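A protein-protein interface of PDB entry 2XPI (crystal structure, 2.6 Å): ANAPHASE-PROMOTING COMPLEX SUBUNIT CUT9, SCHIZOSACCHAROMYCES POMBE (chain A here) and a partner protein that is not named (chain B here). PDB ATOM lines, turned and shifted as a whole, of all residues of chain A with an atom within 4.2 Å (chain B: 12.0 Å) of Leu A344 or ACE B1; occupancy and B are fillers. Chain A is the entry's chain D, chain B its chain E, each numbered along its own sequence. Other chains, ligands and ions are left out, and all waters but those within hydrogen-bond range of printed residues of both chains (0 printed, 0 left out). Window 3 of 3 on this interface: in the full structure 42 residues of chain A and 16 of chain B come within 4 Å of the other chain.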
ATOM      1  N   LEU A 309       6.199  10.903  26.872  1.00  0.00           N
ATOM      2  CA  LEU A 309       6.186  12.323  27.157  1.00  0.00           C
ATOM      3  C   LEU A 309       7.291  12.631  28.146  1.00  0.00           C
ATOM      4  O   LEU A 309       7.869  13.716  28.153  1.00  0.00           O
ATOM      5  CB  LEU A 309       4.836  12.701  27.757  1.00  0.00           C
ATOM      6  CG  LEU A 309       4.298  14.106  27.520  1.00  0.00           C
ATOM      7  CD1 LEU A 309       5.092  14.776  26.420  1.00  0.00           C
ATOM      8  CD2 LEU A 309       2.789  14.050  27.178  1.00  0.00           C
ATOM      9  N   ALA A 312      10.653  12.599  26.160  1.00  0.00           N
ATOM     10  CA  ALA A 312      10.860  13.826  25.414  1.00  0.00           C
ATOM     11  C   ALA A 312      11.172  15.025  26.319  1.00  0.00           C
ATOM     12  O   ALA A 312      11.881  15.938  25.901  1.00  0.00           O
ATOM     13  CB  ALA A 312       9.656  14.116  24.516  1.00  0.00           C
ATOM     14  N   ASP A 313      10.641  15.034  27.542  1.00  0.00           N
ATOM     15  CA  ASP A 313      10.981  16.085  28.502  1.00  0.00           C
ATOM     16  C   ASP A 313      12.467  16.006  28.805  1.00  0.00           C
ATOM     17  O   ASP A 313      13.167  17.015  28.804  1.00  0.00           O
ATOM     18  CB  ASP A 313      10.200  15.934  29.805  1.00  0.00           C
ATOM     19  CG  ASP A 313       8.728  16.295  29.658  1.00  0.00           C
ATOM     20  OD1 ASP A 313       8.408  17.131  28.778  1.00  0.00           O
ATOM     21  OD2 ASP A 313       7.885  15.745  30.425  1.00  0.00           O
ATOM     22  N   PHE A 316      14.394  17.077  25.844  1.00  0.00           N
ATOM     23  CA  PHE A 316      14.347  18.518  25.630  1.00  0.00           C
ATOM     24  C   PHE A 316      15.303  19.269  26.547  1.00  0.00           C
ATOM     25  O   PHE A 316      15.871  20.291  26.164  1.00  0.00           O
ATOM     26  CB  PHE A 316      12.930  19.056  25.825  1.00  0.00           C
ATOM     27  CG  PHE A 316      12.782  20.509  25.472  1.00  0.00           C
ATOM     28  CD1 PHE A 316      12.449  20.889  24.183  1.00  0.00           C
ATOM     29  CD2 PHE A 316      12.975  21.490  26.430  1.00  0.00           C
ATOM     30  CE1 PHE A 316      12.314  22.224  23.850  1.00  0.00           C
ATOM     31  CE2 PHE A 316      12.840  22.826  26.114  1.00  0.00           C
ATOM     32  CZ  PHE A 316      12.503  23.196  24.819  1.00  0.00           C
ATOM     33  N   VAL A 341       0.962  17.294  24.935  1.00  0.00           N
ATOM     34  CA  VAL A 341       2.176  17.236  24.135  1.00  0.00           C
ATOM     35  C   VAL A 341       2.552  18.573  23.463  1.00  0.00           C
ATOM     36  O   VAL A 341       3.711  18.829  23.141  1.00  0.00           O
ATOM     37  CB  VAL A 341       2.012  16.159  23.039  1.00  0.00           C
ATOM     38  CG1 VAL A 341       1.019  16.626  21.983  1.00  0.00           C
ATOM     39  CG2 VAL A 341       3.340  15.815  22.404  1.00  0.00           C
ATOM     40  N   TYR A 342       1.574  19.433  23.244  1.00  0.00           N
ATOM     41  CA  TYR A 342       1.810  20.608  22.416  1.00  0.00           C
ATOM     42  C   TYR A 342       2.892  21.599  22.871  1.00  0.00           C
ATOM     43  O   TYR A 342       3.715  22.015  22.062  1.00  0.00           O
ATOM     44  CB  TYR A 342       0.499  21.314  22.079  1.00  0.00           C
ATOM     45  CG  TYR A 342      -0.228  20.643  20.932  1.00  0.00           C
ATOM     46  CD1 TYR A 342       0.308  20.667  19.655  1.00  0.00           C
ATOM     47  CD2 TYR A 342      -1.442  19.976  21.128  1.00  0.00           C
ATOM     48  CE1 TYR A 342      -0.339  20.058  18.594  1.00  0.00           C
ATOM     49  CE2 TYR A 342      -2.098  19.362  20.074  1.00  0.00           C
ATOM     50  CZ  TYR A 342      -1.539  19.405  18.804  1.00  0.00           C
ATOM     51  OH  TYR A 342      -2.156  18.797  17.721  1.00  0.00           O
ATOM     52  N   PRO A 343       2.903  21.996  24.152  1.00  0.00           N
ATOM     53  CA  PRO A 343       3.899  23.030  24.462  1.00  0.00           C
ATOM     54  C   PRO A 343       5.322  22.585  24.113  1.00  0.00           C
ATOM     55  O   PRO A 343       6.149  23.391  23.709  1.00  0.00           O
ATOM     56  CB  PRO A 343       3.736  23.223  25.976  1.00  0.00           C
ATOM     57  CG  PRO A 343       2.330  22.783  26.257  1.00  0.00           C
ATOM     58  CD  PRO A 343       2.071  21.654  25.321  1.00  0.00           C
ATOM     59  N   LEU A 344       5.579  21.294  24.261  1.00  0.00           N
ATOM     60  CA  LEU A 344       6.879  20.709  23.980  1.00  0.00           C
ATOM     61  C   LEU A 344       7.093  20.572  22.482  1.00  0.00           C
ATOM     62  O   LEU A 344       8.196  20.771  21.973  1.00  0.00           O
ATOM     63  CB  LEU A 344       6.933  19.330  24.614  1.00  0.00           C
ATOM     64  CG  LEU A 344       8.303  18.725  24.831  1.00  0.00           C
ATOM     65  CD1 LEU A 344       9.182  19.752  25.503  1.00  0.00           C
ATOM     66  CD2 LEU A 344       8.131  17.485  25.683  1.00  0.00           C
ATOM     67  N   HIS A 345       6.026  20.218  21.773  1.00  0.00           N
ATOM     68  CA  HIS A 345       6.090  20.096  20.327  1.00  0.00           C
ATOM     69  C   HIS A 345       6.273  21.463  19.657  1.00  0.00           C
ATOM     70  O   HIS A 345       7.124  21.627  18.785  1.00  0.00           O
ATOM     71  CB  HIS A 345       4.835  19.406  19.810  1.00  0.00           C
ATOM     72  CG  HIS A 345       4.927  18.981  18.379  1.00  0.00           C
ATOM     73  ND1 HIS A 345       4.478  19.766  17.337  1.00  0.00           N
ATOM     74  CD2 HIS A 345       5.405  17.849  17.817  1.00  0.00           C
ATOM     75  CE1 HIS A 345       4.676  19.131  16.196  1.00  0.00           C
ATOM     76  NE2 HIS A 345       5.234  17.965  16.460  1.00  0.00           N
ATOM     77  N   LEU A 346       5.469  22.437  20.074  1.00  0.00           N
ATOM     78  CA  LEU A 346       5.607  23.811  19.608  1.00  0.00           C
ATOM     79  C   LEU A 346       6.990  24.401  19.933  1.00  0.00           C
ATOM     80  O   LEU A 346       7.629  25.022  19.069  1.00  0.00           O
ATOM     81  CB  LEU A 346       4.514  24.701  20.218  1.00  0.00           C
ATOM     82  CG  LEU A 346       3.068  24.756  19.692  1.00  0.00           C
ATOM     83  CD1 LEU A 346       2.874  24.145  18.294  1.00  0.00           C
ATOM     84  CD2 LEU A 346       2.102  24.154  20.697  1.00  0.00           C
ATOM     85  N   ALA A 347       7.449  24.232  21.172  1.00  0.00           N
ATOM     86  CA  ALA A 347       8.769  24.758  21.544  1.00  0.00           C
ATOM     87  C   ALA A 347       9.891  24.162  20.675  1.00  0.00           C
ATOM     88  O   ALA A 347      10.721  24.902  20.138  1.00  0.00           O
ATOM     89  CB  ALA A 347       9.055  24.562  23.030  1.00  0.00           C
ATOM     90  N   SER A 348       9.900  22.836  20.531  1.00  0.00           N
ATOM     91  CA  SER A 348      10.841  22.154  19.635  1.00  0.00           C
ATOM     92  C   SER A 348      10.781  22.592  18.158  1.00  0.00           C
ATOM     93  O   SER A 348      11.809  22.639  17.477  1.00  0.00           O
ATOM     94  CB  SER A 348      10.655  20.642  19.714  1.00  0.00           C
ATOM     95  OG  SER A 348      10.779  20.204  21.049  1.00  0.00           O
ATOM     96  N   PRO A 408       4.102  27.974  29.998  1.00  0.00           N
ATOM     97  CA  PRO A 408       4.662  28.190  28.658  1.00  0.00           C
ATOM     98  C   PRO A 408       4.275  29.529  28.021  1.00  0.00           C
ATOM     99  O   PRO A 408       5.040  30.065  27.212  1.00  0.00           O
ATOM    100  CB  PRO A 408       4.083  27.027  27.854  1.00  0.00           C
ATOM    101  CG  PRO A 408       3.897  25.932  28.866  1.00  0.00           C
ATOM    102  CD  PRO A 408       3.551  26.614  30.163  1.00  0.00           C
ATOM    103  C   ACE B   1       8.238  23.971  26.927  1.00  0.00           C
ATOM    104  O   ACE B   1       7.249  24.656  26.612  1.00  0.00           O
ATOM    105  CH3 ACE B   1       8.142  22.490  27.101  1.00  0.00           C
ATOM    106  N   MET B   2       9.390  24.524  27.071  1.00  0.00           N
ATOM    107  CA  MET B   2       9.645  25.951  27.167  1.00  0.00           C
ATOM    108  C   MET B   2      10.478  26.544  26.023  1.00  0.00           C
ATOM    109  O   MET B   2      11.509  26.000  25.636  1.00  0.00           O
ATOM    110  CB  MET B   2      10.386  26.165  28.465  1.00  0.00           C
ATOM    111  CG  MET B   2      10.198  27.469  29.148  1.00  0.00           C
ATOM    112  SD  MET B   2      10.561  27.037  30.850  1.00  0.00           S
ATOM    113  CE  MET B   2      11.126  28.618  31.471  1.00  0.00           C
ATOM    114  N   LEU B   3      10.011  27.664  25.484  1.00  0.00           N
ATOM    115  CA  LEU B   3      10.763  28.433  24.515  1.00  0.00           C
ATOM    116  C   LEU B   3      12.103  28.861  25.095  1.00  0.00           C
ATOM    117  O   LEU B   3      12.173  29.399  26.196  1.00  0.00           O
ATOM    118  CB  LEU B   3       9.996  29.691  24.130  1.00  0.00           C
ATOM    119  CG  LEU B   3       9.075  29.634  22.916  1.00  0.00           C
ATOM    120  CD1 LEU B   3       8.607  28.210  22.679  1.00  0.00           C
ATOM    121  CD2 LEU B   3       7.893  30.584  23.083  1.00  0.00           C
ATOM    122  N   ARG B   4      13.165  28.654  24.329  1.00  0.00           N
ATOM    123  CA  ARG B   4      14.478  29.106  24.731  1.00  0.00           C
ATOM    124  C   ARG B   4      14.790  30.421  24.056  1.00  0.00           C
ATOM    125  O   ARG B   4      13.997  30.938  23.289  1.00  0.00           O
ATOM    126  CB  ARG B   4      15.530  28.073  24.335  1.00  0.00           C
ATOM    127  CG  ARG B   4      15.223  26.692  24.820  1.00  0.00           C
ATOM    128  CD  ARG B   4      16.304  25.748  24.380  1.00  0.00           C
ATOM    129  NE  ARG B   4      16.811  25.051  25.549  1.00  0.00           N
ATOM    130  CZ  ARG B   4      17.909  25.389  26.215  1.00  0.00           C
ATOM    131  NH1 ARG B   4      18.665  26.389  25.801  1.00  0.00           N
ATOM    132  NH2 ARG B   4      18.251  24.700  27.285  1.00  0.00           N
ATOM    133  N   ARG B   5      15.951  30.972  24.352  1.00  0.00           N
ATOM    134  CA  ARG B   5      16.457  32.083  23.577  1.00  0.00           C
ATOM    135  C   ARG B   5      17.944  31.924  23.329  1.00  0.00           C
ATOM    136  O   ARG B   5      18.549  30.939  23.754  1.00  0.00           O
ATOM    137  CB  ARG B   5      16.153  33.411  24.252  1.00  0.00           C
ATOM    138  CG  ARG B   5      16.330  33.407  25.727  1.00  0.00           C
ATOM    139  CD  ARG B   5      15.650  34.629  26.306  1.00  0.00           C
ATOM    140  NE  ARG B   5      16.368  35.864  26.023  1.00  0.00           N
ATOM    141  CZ  ARG B   5      16.454  36.870  26.887  1.00  0.00           C
ATOM    142  NH1 ARG B   5      15.865  36.770  28.084  1.00  0.00           N
ATOM    143  NH2 ARG B   5      17.120  37.973  26.565  1.00  0.00           N
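O of ACE B1 sits close to the backbone carbonyl oxygen (O) of Pro A343, at 3.4 Å.
The backbone carbonyl oxygen (O) of Leu A344 lies within hydrogen-bond range of the side-chain hydroxyl (OG) of Ser A348 (2.8 Å).
Among the printed residues, pairs that only touch across the chains: Phe A316 with Met B2 (3.1 Å), Leu A344 with ACE B1 (3.3 Å), Ala A347 with Leu B3 (3.6 Å) and Ala A347 with Met B2 (3.9 Å).
No residue of chain B comes within 4 Å of Leu A309.
No residue of chain B comes within 4 Å of Asp A313.
Of chain B, only Met B2 (3.1 Å) comes within 4 Å of Phe A316.
Val A341 touches none of the printed residues of chain B.
Of the printed residues of chain B, Pro A343 touches ACE B1 (3.4 Å).
Leu A344 touches one residue of chain B.
No residue of chain B comes within 4 Å of His A345.
No residue of chain B comes within 4 Å of Leu A346.
Of the printed residues of chain B, Ala A347 touches Met B2 (3.9 Å) and Leu B3 (3.6 Å).
Ser A348 touches none of the printed residues of chain B.
Of the printed residues of chain A, Met B2 touches Phe A316 and Ala A347.
Printed residues of chain A within 4 Å of Leu B3: Ala A347.
The nearest residue of chain B that does not touch Leu A344 is Met B2 (5.0 Å).
The nearest printed residue of chain A that does not touch ACE B1 is Ala A347 (4.01 Å).
The nearest printed residue of chain B that does not touch Ala A347 is ACE B1 (4.01 Å).
Of the 13 printed residues of chain A, 4 touch a printed residue of chain B.
Printed residues of chain A that touch a printed residue of chain B: Phe A316, Pro A343, Leu A344 and Ala A347.
Hydrophobic or aromatic side chains of chain A that line the printed part of chain B: Phe A316, Pro A343, Leu A344 and Ala A347.
Among the printed residues, 5 pairs touch across the chains.
Among the printed residues, no Asp or Glu carboxylate lies within 4 Å of a Lys or Arg side-chain nitrogen of the other chain.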
